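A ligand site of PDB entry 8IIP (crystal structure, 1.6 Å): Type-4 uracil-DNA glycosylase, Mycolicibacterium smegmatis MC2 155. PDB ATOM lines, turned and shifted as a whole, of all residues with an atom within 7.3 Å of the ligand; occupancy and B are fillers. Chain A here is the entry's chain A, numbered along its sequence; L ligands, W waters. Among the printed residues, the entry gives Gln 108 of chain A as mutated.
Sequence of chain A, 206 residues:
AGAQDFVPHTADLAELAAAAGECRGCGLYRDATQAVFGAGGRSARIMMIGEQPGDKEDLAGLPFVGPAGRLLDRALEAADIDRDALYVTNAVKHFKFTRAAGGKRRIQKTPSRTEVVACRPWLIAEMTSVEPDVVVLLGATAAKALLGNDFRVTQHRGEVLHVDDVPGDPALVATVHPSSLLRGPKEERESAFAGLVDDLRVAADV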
ATOM      1  N   VAL A  36     -19.457  29.792 -25.864  1.00  0.00           N
ATOM      2  CA  VAL A  36     -20.381  28.727 -25.509  1.00  0.00           C
ATOM      3  C   VAL A  36     -21.639  28.980 -26.334  1.00  0.00           C
ATOM      4  O   VAL A  36     -22.457  29.837 -25.973  1.00  0.00           O
ATOM      5  CB  VAL A  36     -20.692  28.697 -24.014  1.00  0.00           C
ATOM      6  CG1 VAL A  36     -21.743  27.601 -23.721  1.00  0.00           C
ATOM      7  CG2 VAL A  36     -19.424  28.461 -23.185  1.00  0.00           C
ATOM      8  N   ILE A  49     -33.348  30.834 -23.296  1.00  0.00           N
ATOM      9  CA  ILE A  49     -32.211  31.762 -23.333  1.00  0.00           C
ATOM     10  C   ILE A  49     -31.886  32.188 -21.916  1.00  0.00           C
ATOM     11  O   ILE A  49     -32.720  32.815 -21.247  1.00  0.00           O
ATOM     12  CB  ILE A  49     -32.510  32.997 -24.207  1.00  0.00           C
ATOM     13  CG1 ILE A  49     -33.005  32.567 -25.599  1.00  0.00           C
ATOM     14  CG2 ILE A  49     -31.282  33.923 -24.308  1.00  0.00           C
ATOM     15  CD1 ILE A  49     -33.411  33.744 -26.461  1.00  0.00           C
ATOM     16  N   GLY A  50     -30.677  31.864 -21.460  1.00  0.00           N
ATOM     17  CA  GLY A  50     -30.146  32.347 -20.177  1.00  0.00           C
ATOM     18  C   GLY A  50     -29.321  33.602 -20.356  1.00  0.00           C
ATOM     19  O   GLY A  50     -29.389  34.285 -21.380  1.00  0.00           O
ATOM     20  N   GLU A  51     -28.512  33.919 -19.332  1.00  0.00           N
ATOM     21  CA  GLU A  51     -27.740  35.164 -19.348  1.00  0.00           C
ATOM     22  C   GLU A  51     -26.408  34.983 -20.064  1.00  0.00           C
ATOM     23  O   GLU A  51     -26.123  35.678 -21.042  1.00  0.00           O
ATOM     24  CB  GLU A  51     -27.514  35.643 -17.914  1.00  0.00           C
ATOM     25  CG  GLU A  51     -26.632  36.877 -17.846  1.00  0.00           C
ATOM     26  CD  GLU A  51     -26.513  37.424 -16.448  1.00  0.00           C
ATOM     27  OE1 GLU A  51     -25.616  36.961 -15.705  1.00  0.00           O
ATOM     28  OE2 GLU A  51     -27.305  38.318 -16.108  1.00  0.00           O
ATOM     29  N   GLN A  52     -25.586  34.060 -19.577  1.00  0.00           N
ATOM     30  CA  GLN A  52     -24.228  33.857 -20.073  1.00  0.00           C
ATOM     31  C   GLN A  52     -23.730  32.521 -19.540  1.00  0.00           C
ATOM     32  O   GLN A  52     -24.287  31.994 -18.580  1.00  0.00           O
ATOM     33  CB  GLN A  52     -23.294  34.977 -19.606  1.00  0.00           C
ATOM     34  CG  GLN A  52     -23.096  34.937 -18.097  1.00  0.00           C
ATOM     35  CD  GLN A  52     -22.001  35.831 -17.653  1.00  0.00           C
ATOM     36  OE1 GLN A  52     -20.891  35.754 -18.188  1.00  0.00           O
ATOM     37  NE2 GLN A  52     -22.287  36.715 -16.702  1.00  0.00           N
ATOM     38  N   PRO A  53     -22.696  31.950 -20.140  1.00  0.00           N
ATOM     39  CA  PRO A  53     -22.096  30.762 -19.536  1.00  0.00           C
ATOM     40  C   PRO A  53     -21.517  31.128 -18.175  1.00  0.00           C
ATOM     41  O   PRO A  53     -21.080  32.261 -17.956  1.00  0.00           O
ATOM     42  CB  PRO A  53     -21.011  30.340 -20.529  1.00  0.00           C
ATOM     43  CG  PRO A  53     -20.744  31.506 -21.372  1.00  0.00           C
ATOM     44  CD  PRO A  53     -21.979  32.389 -21.355  1.00  0.00           C
ATOM     45  N   GLY A  54     -21.583  30.179 -17.242  1.00  0.00           N
ATOM     46  CA  GLY A  54     -20.896  30.294 -15.970  1.00  0.00           C
ATOM     47  C   GLY A  54     -19.551  29.589 -16.005  1.00  0.00           C
ATOM     48  O   GLY A  54     -19.061  29.178 -17.061  1.00  0.00           O
ATOM     49  N   ASP A  55     -18.948  29.445 -14.823  1.00  0.00           N
ATOM     50  CA  ASP A  55     -17.622  28.843 -14.705  1.00  0.00           C
ATOM     51  C   ASP A  55     -17.568  27.451 -15.344  1.00  0.00           C
ATOM     52  O   ASP A  55     -16.674  27.148 -16.137  1.00  0.00           O
ATOM     53  CB  ASP A  55     -17.265  28.811 -13.212  1.00  0.00           C
ATOM     54  CG  ASP A  55     -15.880  28.251 -12.922  1.00  0.00           C
ATOM     55  OD1 ASP A  55     -15.109  27.855 -13.824  1.00  0.00           O
ATOM     56  OD2 ASP A  55     -15.561  28.226 -11.714  1.00  0.00           O
ATOM     57  N   GLU A  57     -19.710  26.087 -17.518  1.00  0.00           N
ATOM     58  CA  GLU A  57     -20.043  26.137 -18.942  1.00  0.00           C
ATOM     59  C   GLU A  57     -18.859  26.583 -19.779  1.00  0.00           C
ATOM     60  O   GLU A  57     -18.665  26.111 -20.906  1.00  0.00           O
ATOM     61  CB  GLU A  57     -21.229  27.084 -19.164  1.00  0.00           C
ATOM     62  CG  GLU A  57     -22.555  26.561 -18.655  1.00  0.00           C
ATOM     63  CD  GLU A  57     -22.768  26.675 -17.163  1.00  0.00           C
ATOM     64  OE1 GLU A  57     -22.029  27.420 -16.484  1.00  0.00           O
ATOM     65  OE2 GLU A  57     -23.690  25.998 -16.669  1.00  0.00           O
ATOM     66  N   LEU A  62     -20.750  23.955 -23.194  1.00  0.00           N
ATOM     67  CA  LEU A  62     -22.187  23.679 -23.256  1.00  0.00           C
ATOM     68  C   LEU A  62     -22.905  24.560 -22.253  1.00  0.00           C
ATOM     69  O   LEU A  62     -22.375  24.820 -21.162  1.00  0.00           O
ATOM     70  CB  LEU A  62     -22.505  22.213 -22.902  1.00  0.00           C
ATOM     71  CG  LEU A  62     -21.921  21.104 -23.765  1.00  0.00           C
ATOM     72  CD1 LEU A  62     -22.107  19.763 -23.069  1.00  0.00           C
ATOM     73  CD2 LEU A  62     -22.622  21.107 -25.108  1.00  0.00           C
ATOM     74  N   PRO A  63     -24.123  25.004 -22.552  1.00  0.00           N
ATOM     75  CA  PRO A  63     -24.865  25.799 -21.576  1.00  0.00           C
ATOM     76  C   PRO A  63     -25.495  24.945 -20.494  1.00  0.00           C
ATOM     77  O   PRO A  63     -25.772  23.751 -20.686  1.00  0.00           O
ATOM     78  CB  PRO A  63     -25.964  26.471 -22.419  1.00  0.00           C
ATOM     79  CG  PRO A  63     -26.140  25.564 -23.605  1.00  0.00           C
ATOM     80  CD  PRO A  63     -24.833  24.848 -23.845  1.00  0.00           C
ATOM     81  N   PHE A  64     -25.699  25.581 -19.340  1.00  0.00           N
ATOM     82  CA  PHE A  64     -26.524  25.076 -18.227  1.00  0.00           C
ATOM     83  C   PHE A  64     -26.100  23.668 -17.811  1.00  0.00           C
ATOM     84  O   PHE A  64     -26.885  22.707 -17.826  1.00  0.00           O
ATOM     85  CB  PHE A  64     -28.010  25.157 -18.586  1.00  0.00           C
ATOM     86  CG  PHE A  64     -28.619  26.527 -18.356  1.00  0.00           C
ATOM     87  CD1 PHE A  64     -28.722  27.050 -17.070  1.00  0.00           C
ATOM     88  CD2 PHE A  64     -29.030  27.311 -19.431  1.00  0.00           C
ATOM     89  CE1 PHE A  64     -29.249  28.318 -16.855  1.00  0.00           C
ATOM     90  CE2 PHE A  64     -29.555  28.580 -19.226  1.00  0.00           C
ATOM     91  CZ  PHE A  64     -29.670  29.085 -17.934  1.00  0.00           C
ATOM     92  N   VAL A  65     -24.824  23.557 -17.419  1.00  0.00           N
ATOM     93  CA  VAL A  65     -24.253  22.288 -16.955  1.00  0.00           C
ATOM     94  C   VAL A  65     -23.910  22.326 -15.477  1.00  0.00           C
ATOM     95  O   VAL A  65     -23.489  21.298 -14.924  1.00  0.00           O
ATOM     96  CB  VAL A  65     -23.006  21.884 -17.767  1.00  0.00           C
ATOM     97  CG1 VAL A  65     -23.408  21.541 -19.201  1.00  0.00           C
ATOM     98  CG2 VAL A  65     -21.944  22.983 -17.708  1.00  0.00           C
ATOM     99  N   GLY A  66     -24.081  23.472 -14.810  1.00  0.00           N
ATOM    100  CA  GLY A  66     -23.741  23.624 -13.412  1.00  0.00           C
ATOM    101  C   GLY A  66     -24.978  23.572 -12.529  1.00  0.00           C
ATOM    102  O   GLY A  66     -26.010  23.014 -12.909  1.00  0.00           O
ATOM    103  N   PRO A  67     -24.868  24.136 -11.326  1.00  0.00           N
ATOM    104  CA  PRO A  67     -25.991  24.074 -10.379  1.00  0.00           C
ATOM    105  C   PRO A  67     -27.296  24.628 -10.931  1.00  0.00           C
ATOM    106  O   PRO A  67     -28.355  24.020 -10.745  1.00  0.00           O
ATOM    107  CB  PRO A  67     -25.464  24.915  -9.209  1.00  0.00           C
ATOM    108  CG  PRO A  67     -24.000  24.556  -9.207  1.00  0.00           C
ATOM    109  CD  PRO A  67     -23.654  24.668 -10.685  1.00  0.00           C
ATOM    110  N   ALA A  68     -27.247  25.790 -11.584  1.00  0.00           N
ATOM    111  CA  ALA A  68     -28.452  26.337 -12.197  1.00  0.00           C
ATOM    112  C   ALA A  68     -29.028  25.387 -13.237  1.00  0.00           C
ATOM    113  O   ALA A  68     -30.250  25.239 -13.361  1.00  0.00           O
ATOM    114  CB  ALA A  68     -28.146  27.700 -12.823  1.00  0.00           C
ATOM    115  N   GLY A  69     -28.160  24.731 -14.016  1.00  0.00           N
ATOM    116  CA  GLY A  69     -28.624  23.779 -15.021  1.00  0.00           C
ATOM    117  C   GLY A  69     -29.277  22.559 -14.411  1.00  0.00           C
ATOM    118  O   GLY A  69     -30.246  22.029 -14.959  1.00  0.00           O
ATOM    119  N   ARG A  83     -35.561  18.007 -22.246  1.00  0.00           N
ATOM    120  CA  ARG A  83     -34.436  18.978 -22.436  1.00  0.00           C
ATOM    121  C   ARG A  83     -33.759  18.694 -23.777  1.00  0.00           C
ATOM    122  O   ARG A  83     -33.186  19.600 -24.401  1.00  0.00           O
ATOM    123  CB  ARG A  83     -33.401  18.873 -21.311  1.00  0.00           C
ATOM    124  CG  ARG A  83     -32.287  19.913 -21.371  1.00  0.00           C
ATOM    125  CD  ARG A  83     -31.013  19.481 -20.668  1.00  0.00           C
ATOM    126  NE  ARG A  83     -29.872  20.348 -20.907  1.00  0.00           N
ATOM    127  CZ  ARG A  83     -29.404  21.267 -20.070  1.00  0.00           C
ATOM    128  NH1 ARG A  83     -29.988  21.470 -18.904  1.00  0.00           N
ATOM    129  NH2 ARG A  83     -28.356  21.998 -20.397  1.00  0.00           N
ATOM    130  N   VAL A  88     -31.178  25.437 -26.310  1.00  0.00           N
ATOM    131  CA  VAL A  88     -30.837  26.174 -25.099  1.00  0.00           C
ATOM    132  C   VAL A  88     -29.598  26.997 -25.385  1.00  0.00           C
ATOM    133  O   VAL A  88     -28.590  26.455 -25.843  1.00  0.00           O
ATOM    134  CB  VAL A  88     -30.594  25.212 -23.917  1.00  0.00           C
ATOM    135  CG1 VAL A  88     -30.124  25.975 -22.676  1.00  0.00           C
ATOM    136  CG2 VAL A  88     -31.858  24.404 -23.635  1.00  0.00           C
ATOM    137  N   THR A  89     -29.654  28.307 -25.086  1.00  0.00           N
ATOM    138  CA  THR A  89     -28.532  29.193 -25.358  1.00  0.00           C
ATOM    139  C   THR A  89     -28.547  30.314 -24.321  1.00  0.00           C
ATOM    140  O   THR A  89     -29.280  30.245 -23.333  1.00  0.00           O
ATOM    141  CB  THR A  89     -28.598  29.720 -26.812  1.00  0.00           C
ATOM    142  OG1 THR A  89     -27.363  30.342 -27.175  1.00  0.00           O
ATOM    143  CG2 THR A  89     -29.785  30.689 -27.021  1.00  0.00           C
ATOM    144  N   ASN A  90     -27.723  31.343 -24.537  1.00  0.00           N
ATOM    145  CA  ASN A  90     -27.552  32.455 -23.606  1.00  0.00           C
ATOM    146  C   ASN A  90     -27.505  33.757 -24.397  1.00  0.00           C
ATOM    147  O   ASN A  90     -27.119  33.773 -25.569  1.00  0.00           O
ATOM    148  CB  ASN A  90     -26.266  32.327 -22.781  1.00  0.00           C
ATOM    149  CG  ASN A  90     -26.353  31.233 -21.736  1.00  0.00           C
ATOM    150  OD1 ASN A  90     -27.204  31.256 -20.854  1.00  0.00           O
ATOM    151  ND2 ASN A  90     -25.481  30.229 -21.856  1.00  0.00           N
ATOM    152  N   ALA A  91     -27.847  34.856 -23.721  1.00  0.00           N
ATOM    153  CA  ALA A  91     -27.812  36.168 -24.380  1.00  0.00           C
ATOM    154  C   ALA A  91     -26.389  36.549 -24.772  1.00  0.00           C
ATOM    155  O   ALA A  91     -26.168  37.202 -25.810  1.00  0.00           O
ATOM    156  CB  ALA A  91     -28.405  37.220 -23.454  1.00  0.00           C
ATOM    157  N   VAL A  92     -25.415  36.197 -23.937  1.00  0.00           N
ATOM    158  CA  VAL A  92     -24.003  36.477 -24.179  1.00  0.00           C
ATOM    159  C   VAL A  92     -23.264  35.148 -24.243  1.00  0.00           C
ATOM    160  O   VAL A  92     -23.581  34.229 -23.484  1.00  0.00           O
ATOM    161  CB  VAL A  92     -23.501  37.402 -23.056  1.00  0.00           C
ATOM    162  CG1 VAL A  92     -21.984  37.401 -22.907  1.00  0.00           C
ATOM    163  CG2 VAL A  92     -24.072  38.825 -23.285  1.00  0.00           C
ATOM    164  N   GLN A 108     -19.366  34.965 -11.801  1.00  0.00           N
ATOM    165  CA  GLN A 108     -19.952  35.649 -12.976  1.00  0.00           C
ATOM    166  C   GLN A 108     -20.089  37.135 -12.683  1.00  0.00           C
ATOM    167  O   GLN A 108     -20.387  37.475 -11.543  1.00  0.00           O
ATOM    168  CB  GLN A 108     -21.380  35.193 -13.284  1.00  0.00           C
ATOM    169  CG  GLN A 108     -21.524  33.920 -14.095  1.00  0.00           C
ATOM    170  CD  GLN A 108     -22.957  33.464 -14.198  1.00  0.00           C
ATOM    171  OE1 GLN A 108     -23.747  33.655 -13.283  1.00  0.00           O
ATOM    172  NE2 GLN A 108     -23.310  32.865 -15.323  1.00  0.00           N
ATOM    173  N   LEU A 138     -34.887  33.369 -19.522  1.00  0.00           N
ATOM    174  CA  LEU A 138     -34.557  33.013 -18.135  1.00  0.00           C
ATOM    175  C   LEU A 138     -33.795  34.172 -17.525  1.00  0.00           C
ATOM    176  O   LEU A 138     -32.584  34.317 -17.754  1.00  0.00           O
ATOM    177  CB  LEU A 138     -33.723  31.725 -18.111  1.00  0.00           C
ATOM    178  CG  LEU A 138     -34.380  30.469 -18.711  1.00  0.00           C
ATOM    179  CD1 LEU A 138     -33.317  29.390 -18.922  1.00  0.00           C
ATOM    180  CD2 LEU A 138     -35.467  29.933 -17.781  1.00  0.00           C
ATOM    181  N   ALA A 142     -31.541  38.105 -20.197  1.00  0.00           N
ATOM    182  CA  ALA A 142     -32.140  37.495 -21.376  1.00  0.00           C
ATOM    183  C   ALA A 142     -33.444  38.170 -21.748  1.00  0.00           C
ATOM    184  O   ALA A 142     -33.704  38.458 -22.922  1.00  0.00           O
ATOM    185  CB  ALA A 142     -32.378  36.005 -21.111  1.00  0.00           C
ATOM    186  N   HIS A 177     -34.677  33.411 -13.357  1.00  0.00           N
ATOM    187  CA  HIS A 177     -33.471  32.648 -13.654  1.00  0.00           C
ATOM    188  C   HIS A 177     -33.321  31.511 -12.647  1.00  0.00           C
ATOM    189  O   HIS A 177     -33.485  31.736 -11.440  1.00  0.00           O
ATOM    190  CB  HIS A 177     -32.244  33.550 -13.604  1.00  0.00           C
ATOM    191  CG  HIS A 177     -31.040  32.940 -14.244  1.00  0.00           C
ATOM    192  ND1 HIS A 177     -30.320  31.932 -13.645  1.00  0.00           N
ATOM    193  CD2 HIS A 177     -30.432  33.185 -15.423  1.00  0.00           C
ATOM    194  CE1 HIS A 177     -29.322  31.568 -14.433  1.00  0.00           C
ATOM    195  NE2 HIS A 177     -29.366  32.314 -15.527  1.00  0.00           N
ATOM    196  N   PRO A 178     -33.000  30.296 -13.084  1.00  0.00           N
ATOM    197  CA  PRO A 178     -32.876  29.184 -12.120  1.00  0.00           C
ATOM    198  C   PRO A 178     -31.837  29.428 -11.036  1.00  0.00           C
ATOM    199  O   PRO A 178     -31.974  28.868  -9.948  1.00  0.00           O
ATOM    200  CB  PRO A 178     -32.510  27.980 -13.000  1.00  0.00           C
ATOM    201  CG  PRO A 178     -32.135  28.546 -14.334  1.00  0.00           C
ATOM    202  CD  PRO A 178     -32.894  29.831 -14.476  1.00  0.00           C
ATOM    203  N   SER A 179     -30.845  30.284 -11.267  1.00  0.00           N
ATOM    204  CA  SER A 179     -29.841  30.601 -10.212  1.00  0.00           C
ATOM    205  C   SER A 179     -30.550  31.230  -9.011  1.00  0.00           C
ATOM    206  O   SER A 179     -30.088  31.029  -7.897  1.00  0.00           O
ATOM    207  CB  SER A 179     -28.767  31.532 -10.706  1.00  0.00           C
ATOM    208  OG  SER A 179     -27.889  30.886 -11.594  1.00  0.00           O
HETATM  209  N1  LIG L   1     -26.362  30.592 -16.163  1.00  0.00           N
HETATM  210  C1  LIG L   1     -26.832  31.031 -17.374  1.00  0.00           C
HETATM  211  O1  LIG L   1     -27.468  32.078 -17.497  1.00  0.00           O
HETATM  212  N2  LIG L   1     -26.509  30.239 -18.450  1.00  0.00           N
HETATM  213  C2  LIG L   1     -25.785  29.067 -18.405  1.00  0.00           C
HETATM  214  O2  LIG L   1     -25.550  28.448 -19.459  1.00  0.00           O
HETATM  215  C3  LIG L   1     -25.342  28.666 -17.093  1.00  0.00           C
HETATM  216  C4  LIG L   1     -25.649  29.442 -16.036  1.00  0.00           C
HETATM  217  O   HOH W   1     -26.387  32.446 -13.857  1.00  0.00           O
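A nitrogen (N2) of the ligand lies within hydrogen-bond range of the side-chain amide oxygen (OD1) of Asn 90, 2.7 Å away.
An oxygen (O1) of the ligand lies within hydrogen-bond range of a ring nitrogen (NE2) of His 177, at 2.7 Å.
The backbone NH (N) of Glu 51 sits at hydrogen-bond distance from an oxygen (O1) of the ligand, 2.8 Å away.
The backbone NH of Gln 52 lies within hydrogen-bond range of an oxygen (O1) of the ligand, 3.4 Å away.
O of Gln 52 is in hydrogen-bond range of N2 of the ligand (2.8 Å).
N of Phe 64 is in hydrogen-bond range of O2 of the ligand.
N of Ser 179 lies within hydrogen-bond range of ND1 of His 177, 2.9 Å away.
The backbone carbonyl oxygen (O) of Glu 51 lies within hydrogen-bond range of the backbone NH (N) of Ala 91, 3.3 Å away.
NH2 of Arg 83 is in hydrogen-bond range of O of Phe 64.
The side-chain carboxylate (OE1) of Glu 57 sits at hydrogen-bond distance from the backbone NH (N) of Gly 54 (2.9 Å).
The side-chain carboxylate of Glu 57 is in hydrogen-bond range of the backbone NH of Val 65.
The side-chain carboxylate (OE2) of Glu 57 is in hydrogen-bond range of the backbone NH (N) of Gly 66 (3.2 Å).
The backbone carbonyl oxygen of Pro 63 is in hydrogen-bond range of the guanidinium group of Arg 83 (3.1 Å).
The backbone carbonyl oxygen (O) of Thr 89 lies within hydrogen-bond range of the backbone NH (N) of Gly 50 (2.8 Å).
Gly 50 touches the ligand.
Glu 57 touches the ligand (OE2 to C3, 3.2 Å).
CA of Pro 63 touches O2 of the ligand (3.5 Å).
NE2 of Gln 108 touches N1 of the ligand (3.9 Å).
Hydrophobic or aromatic side chains that line the ligand: Pro 63, Phe 64 and His 177.
Of the 29 residues printed, 9 come within 4 Å of the ligand.
Along chain A the residues within 4 Å of the ligand span positions 50 to 177.
Water W1 lies within hydrogen-bond range of a nitrogen (N1) of the ligand (3.0 Å), the side-chain amide oxygen of Gln 108 (3.0 Å), the side-chain hydroxyl of Ser 179 (3.1 Å) and a ring nitrogen (NE2) of His 177 (3.4 Å).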
